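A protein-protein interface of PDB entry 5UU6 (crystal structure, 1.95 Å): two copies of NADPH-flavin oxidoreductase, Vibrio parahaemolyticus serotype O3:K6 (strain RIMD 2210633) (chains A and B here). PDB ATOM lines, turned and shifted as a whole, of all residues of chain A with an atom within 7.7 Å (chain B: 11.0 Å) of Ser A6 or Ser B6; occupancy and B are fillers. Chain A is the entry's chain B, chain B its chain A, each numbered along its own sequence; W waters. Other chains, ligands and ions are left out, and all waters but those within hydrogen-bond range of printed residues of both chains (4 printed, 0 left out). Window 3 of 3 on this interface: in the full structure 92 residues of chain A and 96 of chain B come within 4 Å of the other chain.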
ATOM      1  N   MET A   4     -16.078  16.613  18.939  1.00  0.00           N
ATOM      2  CA  MET A   4     -17.254  16.833  18.102  1.00  0.00           C
ATOM      3  C   MET A   4     -18.349  17.601  18.845  1.00  0.00           C
ATOM      4  O   MET A   4     -18.085  18.269  19.848  1.00  0.00           O
ATOM      5  CB  MET A   4     -17.818  15.490  17.618  1.00  0.00           C
ATOM      6  CG  MET A   4     -17.536  15.151  16.158  1.00  0.00           C
ATOM      7  SD  MET A   4     -18.100  16.542  14.897  1.00  0.00           S
ATOM      8  CE  MET A   4     -18.185  15.495  13.236  1.00  0.00           C
ATOM      9  N   ASN A   5     -19.561  17.527  18.292  1.00  0.00           N
ATOM     10  CA  ASN A   5     -20.832  17.628  19.000  1.00  0.00           C
ATOM     11  C   ASN A   5     -21.924  17.445  17.954  1.00  0.00           C
ATOM     12  O   ASN A   5     -21.679  17.532  16.741  1.00  0.00           O
ATOM     13  CB  ASN A   5     -21.018  18.929  19.797  1.00  0.00           C
ATOM     14  CG  ASN A   5     -21.035  20.175  18.917  1.00  0.00           C
ATOM     15  OD1 ASN A   5     -21.761  20.242  17.928  1.00  0.00           O
ATOM     16  ND2 ASN A   5     -20.249  21.180  19.301  1.00  0.00           N
ATOM     17  N   SER A   6     -23.141  17.192  18.434  1.00  0.00           N
ATOM     18  CA  SER A   6     -24.210  16.857  17.499  1.00  0.00           C
ATOM     19  C   SER A   6     -24.620  18.027  16.612  1.00  0.00           C
ATOM     20  O   SER A   6     -25.131  17.788  15.512  1.00  0.00           O
ATOM     21  CB  SER A   6     -25.416  16.291  18.243  1.00  0.00           C
ATOM     22  OG  SER A   6     -25.868  17.205  19.215  1.00  0.00           O
ATOM     23  N   THR A   7     -24.419  19.291  17.024  1.00  0.00           N
ATOM     24  CA  THR A   7     -24.736  20.378  16.084  1.00  0.00           C
ATOM     25  C   THR A   7     -23.794  20.353  14.891  1.00  0.00           C
ATOM     26  O   THR A   7     -24.217  20.540  13.739  1.00  0.00           O
ATOM     27  CB  THR A   7     -24.657  21.749  16.766  1.00  0.00           C
ATOM     28  OG1 THR A   7     -25.561  21.797  17.877  1.00  0.00           O
ATOM     29  CG2 THR A   7     -24.967  22.889  15.764  1.00  0.00           C
ATOM     30  N   ILE A   8     -22.511  20.117  15.136  1.00  0.00           N
ATOM     31  CA  ILE A   8     -21.557  20.117  14.036  1.00  0.00           C
ATOM     32  C   ILE A   8     -21.826  18.948  13.104  1.00  0.00           C
ATOM     33  O   ILE A   8     -21.865  19.101  11.878  1.00  0.00           O
ATOM     34  CB  ILE A   8     -20.117  20.060  14.570  1.00  0.00           C
ATOM     35  CG1 ILE A   8     -19.837  21.198  15.543  1.00  0.00           C
ATOM     36  CG2 ILE A   8     -19.153  20.017  13.394  1.00  0.00           C
ATOM     37  CD1 ILE A   8     -20.021  22.495  14.957  1.00  0.00           C
ATOM     38  N   GLN A   9     -21.981  17.745  13.658  1.00  0.00           N
ATOM     39  CA  GLN A   9     -22.309  16.643  12.758  1.00  0.00           C
ATOM     40  C   GLN A   9     -23.636  16.881  12.052  1.00  0.00           C
ATOM     41  O   GLN A   9     -23.783  16.482  10.894  1.00  0.00           O
ATOM     42  CB  GLN A   9     -22.293  15.299  13.472  1.00  0.00           C
ATOM     43  CG  GLN A   9     -22.732  15.307  14.884  1.00  0.00           C
ATOM     44  CD  GLN A   9     -22.578  13.927  15.553  1.00  0.00           C
ATOM     45  OE1 GLN A   9     -21.551  13.255  15.398  1.00  0.00           O
ATOM     46  NE2 GLN A   9     -23.604  13.508  16.292  1.00  0.00           N
ATOM     47  N   THR A  10     -24.596  17.574  12.674  1.00  0.00           N
ATOM     48  CA  THR A  10     -25.807  17.900  11.910  1.00  0.00           C
ATOM     49  C   THR A  10     -25.473  18.793  10.727  1.00  0.00           C
ATOM     50  O   THR A  10     -25.879  18.512   9.584  1.00  0.00           O
ATOM     51  CB  THR A  10     -26.881  18.567  12.772  1.00  0.00           C
ATOM     52  OG1 THR A  10     -27.381  17.635  13.734  1.00  0.00           O
ATOM     53  CG2 THR A  10     -28.070  18.977  11.876  1.00  0.00           C
ATOM     54  N   ILE A  11     -24.738  19.884  10.983  1.00  0.00           N
ATOM     55  CA  ILE A  11     -24.325  20.804   9.916  1.00  0.00           C
ATOM     56  C   ILE A  11     -23.521  20.071   8.842  1.00  0.00           C
ATOM     57  O   ILE A  11     -23.764  20.228   7.637  1.00  0.00           O
ATOM     58  CB  ILE A  11     -23.524  21.987  10.496  1.00  0.00           C
ATOM     59  CG1 ILE A  11     -24.379  22.838  11.442  1.00  0.00           C
ATOM     60  CG2 ILE A  11     -22.952  22.859   9.363  1.00  0.00           C
ATOM     61  CD1 ILE A  11     -23.584  23.879  12.268  1.00  0.00           C
ATOM     62  N   LEU A  12     -22.536  19.274   9.253  1.00  0.00           N
ATOM     63  CA  LEU A  12     -21.656  18.681   8.246  1.00  0.00           C
ATOM     64  C   LEU A  12     -22.334  17.563   7.479  1.00  0.00           C
ATOM     65  O   LEU A  12     -21.897  17.248   6.367  1.00  0.00           O
ATOM     66  CB  LEU A  12     -20.350  18.152   8.864  1.00  0.00           C
ATOM     67  CG  LEU A  12     -19.396  19.242   9.377  1.00  0.00           C
ATOM     68  CD1 LEU A  12     -18.043  18.650   9.770  1.00  0.00           C
ATOM     69  CD2 LEU A  12     -19.197  20.401   8.398  1.00  0.00           C
ATOM     70  N   GLU A 123     -33.388  19.113  10.553  1.00  0.00           N
ATOM     71  CA  GLU A 123     -32.410  18.058  10.283  1.00  0.00           C
ATOM     72  C   GLU A 123     -31.885  17.449  11.568  1.00  0.00           C
ATOM     73  O   GLU A 123     -31.525  16.259  11.588  1.00  0.00           O
ATOM     74  CB  GLU A 123     -31.240  18.598   9.455  1.00  0.00           C
ATOM     75  CG  GLU A 123     -31.609  19.010   7.995  1.00  0.00           C
ATOM     76  CD  GLU A 123     -30.434  19.623   7.228  1.00  0.00           C
ATOM     77  OE1 GLU A 123     -29.449  20.112   7.848  1.00  0.00           O
ATOM     78  OE2 GLU A 123     -30.485  19.619   5.982  1.00  0.00           O
ATOM     79  N   SER A 124     -31.826  18.251  12.647  1.00  0.00           N
ATOM     80  CA  SER A 124     -31.405  17.749  13.950  1.00  0.00           C
ATOM     81  C   SER A 124     -32.356  16.703  14.480  1.00  0.00           C
ATOM     82  O   SER A 124     -31.966  15.905  15.343  1.00  0.00           O
ATOM     83  CB  SER A 124     -31.302  18.903  14.975  1.00  0.00           C
ATOM     84  OG  SER A 124     -32.562  19.254  15.552  1.00  0.00           O
ATOM     85  N   ALA B   3     -39.076  16.806  21.525  1.00  0.00           N
ATOM     86  CA  ALA B   3     -38.246  17.331  20.416  1.00  0.00           C
ATOM     87  C   ALA B   3     -37.196  18.333  20.924  1.00  0.00           C
ATOM     88  O   ALA B   3     -37.328  19.541  20.703  1.00  0.00           O
ATOM     89  CB  ALA B   3     -39.137  17.988  19.323  1.00  0.00           C
ATOM     90  N   MET B   4     -36.175  17.836  21.626  1.00  0.00           N
ATOM     91  CA  MET B   4     -35.132  18.705  22.194  1.00  0.00           C
ATOM     92  C   MET B   4     -33.764  18.041  22.272  1.00  0.00           C
ATOM     93  O   MET B   4     -33.533  17.113  23.057  1.00  0.00           O
ATOM     94  CB  MET B   4     -35.490  19.175  23.603  1.00  0.00           C
ATOM     95  CG  MET B   4     -34.363  19.982  24.249  1.00  0.00           C
ATOM     96  SD  MET B   4     -34.046  21.679  23.307  1.00  0.00           S
ATOM     97  CE  MET B   4     -35.924  22.278  23.330  1.00  0.00           C
ATOM     98  N   ASN B   5     -32.840  18.563  21.487  1.00  0.00           N
ATOM     99  CA  ASN B   5     -31.488  18.046  21.410  1.00  0.00           C
ATOM    100  C   ASN B   5     -30.572  19.248  21.547  1.00  0.00           C
ATOM    101  O   ASN B   5     -31.048  20.377  21.712  1.00  0.00           O
ATOM    102  CB  ASN B   5     -31.287  17.301  20.093  1.00  0.00           C
ATOM    103  CG  ASN B   5     -31.647  18.176  18.897  1.00  0.00           C
ATOM    104  OD1 ASN B   5     -31.065  19.222  18.728  1.00  0.00           O
ATOM    105  ND2 ASN B   5     -32.632  17.761  18.097  1.00  0.00           N
ATOM    106  N   SER B   6     -29.261  19.039  21.471  1.00  0.00           N
ATOM    107  CA  SER B   6     -28.359  20.163  21.745  1.00  0.00           C
ATOM    108  C   SER B   6     -28.289  21.158  20.580  1.00  0.00           C
ATOM    109  O   SER B   6     -27.902  22.327  20.777  1.00  0.00           O
ATOM    110  CB  SER B   6     -26.962  19.653  22.113  1.00  0.00           C
ATOM    111  OG  SER B   6     -26.337  19.018  21.020  1.00  0.00           O
ATOM    112  N   THR B   7     -28.668  20.736  19.377  1.00  0.00           N
ATOM    113  CA  THR B   7     -28.773  21.700  18.274  1.00  0.00           C
ATOM    114  C   THR B   7     -29.880  22.708  18.542  1.00  0.00           C
ATOM    115  O   THR B   7     -29.673  23.924  18.455  1.00  0.00           O
ATOM    116  CB  THR B   7     -29.041  20.971  16.954  1.00  0.00           C
ATOM    117  OG1 THR B   7     -27.930  20.134  16.643  1.00  0.00           O
ATOM    118  CG2 THR B   7     -29.261  21.970  15.840  1.00  0.00           C
ATOM    119  N   ILE B   8     -31.085  22.204  18.817  1.00  0.00           N
ATOM    120  CA  ILE B   8     -32.208  23.054  19.211  1.00  0.00           C
ATOM    121  C   ILE B   8     -31.844  23.906  20.423  1.00  0.00           C
ATOM    122  O   ILE B   8     -32.191  25.097  20.512  1.00  0.00           O
ATOM    123  CB  ILE B   8     -33.433  22.179  19.523  1.00  0.00           C
ATOM    124  CG1 ILE B   8     -33.761  21.258  18.349  1.00  0.00           C
ATOM    125  CG2 ILE B   8     -34.613  23.039  19.893  1.00  0.00           C
ATOM    126  CD1 ILE B   8     -34.152  21.976  17.152  1.00  0.00           C
ATOM    127  N   GLN B   9     -31.210  23.291  21.410  1.00  0.00           N
ATOM    128  CA  GLN B   9     -30.820  24.057  22.583  1.00  0.00           C
ATOM    129  C   GLN B   9     -29.880  25.203  22.197  1.00  0.00           C
ATOM    130  O   GLN B   9     -30.061  26.336  22.649  1.00  0.00           O
ATOM    131  CB  GLN B   9     -30.187  23.119  23.607  1.00  0.00           C
ATOM    132  CG  GLN B   9     -29.611  23.843  24.815  1.00  0.00           C
ATOM    133  CD  GLN B   9     -28.720  22.934  25.666  1.00  0.00           C
ATOM    134  OE1 GLN B   9     -28.229  21.905  25.199  1.00  0.00           O
ATOM    135  NE2 GLN B   9     -28.513  23.319  26.921  1.00  0.00           N
ATOM    136  N   THR B  10     -28.920  24.952  21.306  1.00  0.00           N
ATOM    137  CA  THR B  10     -28.036  26.031  20.847  1.00  0.00           C
ATOM    138  C   THR B  10     -28.821  27.124  20.106  1.00  0.00           C
ATOM    139  O   THR B  10     -28.611  28.327  20.333  1.00  0.00           O
ATOM    140  CB  THR B  10     -26.933  25.433  19.961  1.00  0.00           C
ATOM    141  OG1 THR B  10     -26.176  24.494  20.739  1.00  0.00           O
ATOM    142  CG2 THR B  10     -25.977  26.526  19.384  1.00  0.00           C
ATOM    143  N   ILE B  11     -29.729  26.721  19.212  1.00  0.00           N
ATOM    144  CA  ILE B  11     -30.461  27.696  18.412  1.00  0.00           C
ATOM    145  C   ILE B  11     -31.283  28.612  19.314  1.00  0.00           C
ATOM    146  O   ILE B  11     -31.217  29.836  19.190  1.00  0.00           O
ATOM    147  CB  ILE B  11     -31.339  26.996  17.359  1.00  0.00           C
ATOM    148  CG1 ILE B  11     -30.464  26.215  16.353  1.00  0.00           C
ATOM    149  CG2 ILE B  11     -32.216  28.006  16.596  1.00  0.00           C
ATOM    150  CD1 ILE B  11     -31.243  25.278  15.403  1.00  0.00           C
ATOM    151  N   LEU B  12     -32.062  28.033  20.232  1.00  0.00           N
ATOM    152  CA  LEU B  12     -32.932  28.805  21.104  1.00  0.00           C
ATOM    153  C   LEU B  12     -32.161  29.590  22.157  1.00  0.00           C
ATOM    154  O   LEU B  12     -32.645  30.626  22.612  1.00  0.00           O
ATOM    155  CB  LEU B  12     -33.955  27.884  21.789  1.00  0.00           C
ATOM    156  CG  LEU B  12     -34.876  27.102  20.860  1.00  0.00           C
ATOM    157  CD1 LEU B  12     -35.879  26.314  21.697  1.00  0.00           C
ATOM    158  CD2 LEU B  12     -35.595  28.022  19.862  1.00  0.00           C
ATOM    159  N   GLY B  13     -30.968  29.145  22.529  1.00  0.00           N
ATOM    160  CA  GLY B  13     -30.149  29.843  23.502  1.00  0.00           C
ATOM    161  C   GLY B  13     -29.298  30.951  22.920  1.00  0.00           C
ATOM    162  O   GLY B  13     -28.401  31.464  23.595  1.00  0.00           O
ATOM    163  N   HIS B  14     -29.560  31.343  21.683  1.00  0.00           N
ATOM    164  CA  HIS B  14     -28.737  32.342  21.007  1.00  0.00           C
ATOM    165  C   HIS B  14     -28.875  33.727  21.629  1.00  0.00           C
ATOM    166  O   HIS B  14     -29.987  34.202  21.862  1.00  0.00           O
ATOM    167  CB  HIS B  14     -29.128  32.447  19.541  1.00  0.00           C
ATOM    168  CG  HIS B  14     -28.632  33.711  18.925  1.00  0.00           C
ATOM    169  ND1 HIS B  14     -27.293  33.929  18.677  1.00  0.00           N
ATOM    170  CD2 HIS B  14     -29.271  34.843  18.561  1.00  0.00           C
ATOM    171  CE1 HIS B  14     -27.130  35.131  18.153  1.00  0.00           C
ATOM    172  NE2 HIS B  14     -28.316  35.710  18.072  1.00  0.00           N
ATOM    173  N   THR B  32     -13.157  24.135  11.955  1.00  0.00           N
ATOM    174  CA  THR B  32     -14.495  23.554  12.013  1.00  0.00           C
ATOM    175  C   THR B  32     -15.577  24.591  11.748  1.00  0.00           C
ATOM    176  O   THR B  32     -16.549  24.303  11.043  1.00  0.00           O
ATOM    177  CB  THR B  32     -14.711  22.908  13.374  1.00  0.00           C
ATOM    178  OG1 THR B  32     -13.745  21.870  13.526  1.00  0.00           O
ATOM    179  CG2 THR B  32     -16.114  22.290  13.499  1.00  0.00           C
ATOM    180  N   ALA B  36     -18.109  24.387   8.670  1.00  0.00           N
ATOM    181  CA  ALA B  36     -19.554  24.341   8.870  1.00  0.00           C
ATOM    182  C   ALA B  36     -20.238  25.291   7.914  1.00  0.00           C
ATOM    183  O   ALA B  36     -21.288  24.967   7.344  1.00  0.00           O
ATOM    184  CB  ALA B  36     -19.924  24.691  10.319  1.00  0.00           C
ATOM    185  N   ASN B 117     -24.611  29.060   9.610  1.00  0.00           N
ATOM    186  CA  ASN B 117     -23.900  27.815   9.893  1.00  0.00           C
ATOM    187  C   ASN B 117     -22.655  28.094  10.714  1.00  0.00           C
ATOM    188  O   ASN B 117     -22.381  27.394  11.692  1.00  0.00           O
ATOM    189  CB  ASN B 117     -23.489  27.084   8.616  1.00  0.00           C
ATOM    190  CG  ASN B 117     -24.526  26.059   8.148  1.00  0.00           C
ATOM    191  OD1 ASN B 117     -25.654  26.007   8.654  1.00  0.00           O
ATOM    192  ND2 ASN B 117     -24.156  25.277   7.128  1.00  0.00           N
ATOM    193  N   LEU B 119     -21.965  30.668  12.658  1.00  0.00           N
ATOM    194  CA  LEU B 119     -22.265  31.158  14.002  1.00  0.00           C
ATOM    195  C   LEU B 119     -22.815  30.050  14.886  1.00  0.00           C
ATOM    196  O   LEU B 119     -22.370  29.890  16.029  1.00  0.00           O
ATOM    197  CB  LEU B 119     -23.246  32.337  13.974  1.00  0.00           C
ATOM    198  CG  LEU B 119     -23.637  32.925  15.343  1.00  0.00           C
ATOM    199  CD1 LEU B 119     -22.452  33.420  16.171  1.00  0.00           C
ATOM    200  CD2 LEU B 119     -24.601  34.076  15.116  1.00  0.00           C
ATOM    201  N   LEU B 120     -23.768  29.259  14.377  1.00  0.00           N
ATOM    202  CA  LEU B 120     -24.283  28.154  15.189  1.00  0.00           C
ATOM    203  C   LEU B 120     -23.188  27.171  15.541  1.00  0.00           C
ATOM    204  O   LEU B 120     -23.175  26.608  16.651  1.00  0.00           O
ATOM    205  CB  LEU B 120     -25.412  27.426  14.454  1.00  0.00           C
ATOM    206  CG  LEU B 120     -26.775  28.097  14.599  1.00  0.00           C
ATOM    207  CD1 LEU B 120     -27.745  27.425  13.665  1.00  0.00           C
ATOM    208  CD2 LEU B 120     -27.282  28.028  16.035  1.00  0.00           C
ATOM    209  N   ALA B 121     -22.298  26.889  14.588  1.00  0.00           N
ATOM    210  CA  ALA B 121     -21.198  26.004  14.900  1.00  0.00           C
ATOM    211  C   ALA B 121     -20.379  26.585  16.053  1.00  0.00           C
ATOM    212  O   ALA B 121     -20.083  25.897  17.029  1.00  0.00           O
ATOM    213  CB  ALA B 121     -20.342  25.781  13.653  1.00  0.00           C
ATOM    214  N   ALA B 122     -20.048  27.866  15.967  1.00  0.00           N
ATOM    215  CA  ALA B 122     -19.302  28.506  17.043  1.00  0.00           C
ATOM    216  C   ALA B 122     -20.063  28.414  18.357  1.00  0.00           C
ATOM    217  O   ALA B 122     -19.505  28.000  19.387  1.00  0.00           O
ATOM    218  CB  ALA B 122     -19.022  29.964  16.691  1.00  0.00           C
ATOM    219  N   GLU B 123     -21.350  28.780  18.335  1.00  0.00           N
ATOM    220  CA  GLU B 123     -22.124  28.787  19.577  1.00  0.00           C
ATOM    221  C   GLU B 123     -22.222  27.389  20.167  1.00  0.00           C
ATOM    222  O   GLU B 123     -22.250  27.228  21.387  1.00  0.00           O
ATOM    223  CB  GLU B 123     -23.514  29.381  19.335  1.00  0.00           C
ATOM    224  CG  GLU B 123     -23.494  30.906  19.124  1.00  0.00           C
ATOM    225  CD  GLU B 123     -24.823  31.470  18.652  1.00  0.00           C
ATOM    226  OE1 GLU B 123     -25.051  32.693  18.845  1.00  0.00           O
ATOM    227  OE2 GLU B 123     -25.640  30.698  18.087  1.00  0.00           O
ATOM    228  N   SER B 124     -22.248  26.361  19.326  1.00  0.00           N
ATOM    229  CA  SER B 124     -22.336  25.010  19.854  1.00  0.00           C
ATOM    230  C   SER B 124     -21.092  24.631  20.662  1.00  0.00           C
ATOM    231  O   SER B 124     -21.175  23.758  21.537  1.00  0.00           O
ATOM    232  CB  SER B 124     -22.567  24.028  18.701  1.00  0.00           C
ATOM    233  OG  SER B 124     -21.340  23.671  18.120  1.00  0.00           O
ATOM    234  N   MET B 125     -19.958  25.287  20.402  1.00  0.00           N
ATOM    235  CA  MET B 125     -18.685  25.063  21.099  1.00  0.00           C
ATOM    236  C   MET B 125     -18.528  25.934  22.339  1.00  0.00           C
ATOM    237  O   MET B 125     -17.476  25.915  22.987  1.00  0.00           O
ATOM    238  CB  MET B 125     -17.502  25.331  20.159  1.00  0.00           C
ATOM    239  CG  MET B 125     -17.437  24.346  18.989  1.00  0.00           C
ATOM    240  SD  MET B 125     -16.210  24.860  17.536  1.00  0.00           S
ATOM    241  CE  MET B 125     -15.400  23.125  17.476  1.00  0.00           C
ATOM    242  N   GLY B 126     -19.566  26.679  22.695  1.00  0.00           N
ATOM    243  CA  GLY B 126     -19.432  27.624  23.780  1.00  0.00           C
ATOM    244  C   GLY B 126     -18.826  28.966  23.394  1.00  0.00           C
ATOM    245  O   GLY B 126     -18.587  29.793  24.283  1.00  0.00           O
HETATM  246  O   HOH W   1     -24.452  20.566  19.919  1.00  0.00           O
HETATM  247  O   HOH W   2     -28.411  16.071  21.191  1.00  0.00           O
HETATM  248  O   HOH W   3     -25.451  22.676   6.557  1.00  0.00           O
HETATM  249  O   HOH W   4     -23.623  17.166  21.566  1.00  0.00           O
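ND2 of Asn B5 lies within hydrogen-bond range of OG of Ser A124, at 3.0 Å. The side-chain hydroxyl of Ser A6 sits at hydrogen-bond distance from the side-chain hydroxyl of Ser B6 (2.6 Å). The side-chain hydroxyl (OG1) of Thr A7 lies within hydrogen-bond range of the side-chain hydroxyl (OG1) of Thr B7 (3.1 Å). The side-chain hydroxyl of Ser B124 lies within hydrogen-bond range of the side-chain amide nitrogen of Asn A5 (3.0 Å).
The side-chain amide oxygen of Asn B5 is in hydrogen-bond range of the backbone NH of Ile B8 (3.0 Å). The side-chain hydroxyl (OG1) of Thr B10 sits at hydrogen-bond distance from the backbone carbonyl oxygen (O) of Ser B6, 2.8 Å away. ND2 of Asn B117 lies within hydrogen-bond range of O of Ala B36 (2.9 Å). The backbone carbonyl oxygen (O) of Ala B121 is in hydrogen-bond range of the side-chain hydroxyl (OG) of Ser B124. The side-chain amide oxygen of Asn A5 lies within hydrogen-bond range of the backbone NH of Thr A7 (3.0 Å). OG1 of Thr A10 sits at hydrogen-bond distance from O of Ser A6, 2.9 Å away.
Thr B7 touches Ser A6. CB of Ser B124 touches CB of Thr A7 (3.6 Å). Thr B32 touches Ile A8 (CG2 to CG2, 3.8 Å). Ile A8 touches Ala B121 (CD1 to CB, 3.5 Å). Ser B124 touches Ile A8. Thr A10 touches Thr B7. ND2 of Asn B117 touches CG2 of Ile A11, at 3.5 Å. Leu A12 touches Ala B36. Thr B7 touches Ser A124. OG of Ser A124 touches CD1 of Ile B8 (3.5 Å).
Ser A6 touches just these residues of chain B: Ser B6 (2.6 Å) and Thr B7 (3.8 Å). Ile A8 touches just these residues of chain B: Thr B32, Ala B121 and Ser B124. No residue of chain B comes within 4 Å of Gln A9. Of the printed residues of chain B, Ile A11 touches Ala B36 (3.4 Å) and Asn B117 (3.5 Å). Of chain A, only Ser A6 (2.6 Å) and Thr A7 (3.8 Å) come within 4 Å of Ser B6. Of the printed residues of chain A, Ala B36 touches Ile A11 (3.4 Å) and Leu A12 (3.98 Å). The nearest printed residue of chain A that does not touch Asn B117 is Ile A8 (6.3 Å).
Of the 23 printed residues of chain B, 10 touch a printed residue of chain A. Hydrophobic or aromatic side chains of chain B that line the printed part of chain A: Ile B8, Ala B36 and Ala B121. Among the printed residues, 17 pairs touch across the chains.
Ser B6 touches its own counterpart, Ser A6. Thr A7 touches its own counterpart, Thr B7. Thr A7 touches Thr B10, and with the chains exchanged Thr A10 touches Thr B7. Thr A7 touches Ser B124, and with the chains exchanged Ser A124 touches Thr B7. Of the 17 pairs that touch across the chains among the printed residues, 12 have their exchanged pair printed and touching as well.
Water W1 lies within hydrogen-bond range of the side-chain hydroxyl (OG1) of Thr A7 (2.6 Å), the side-chain hydroxyl (OG) of Ser B6 (2.7 Å) and the side-chain amide oxygen (OD1) of Asn A5 (3.4 Å). Water W3 bridges ND2 of Asn B117 and O of Ile A11. Water W2 bridges N of Ser B6 (3.1 Å) and OG of Ser A6 (3.4 Å). Water W4 lies within hydrogen-bond range of the backbone NH of Ser A6 (3.2 Å) and the side-chain hydroxyl of Ser B6 (3.3 Å).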
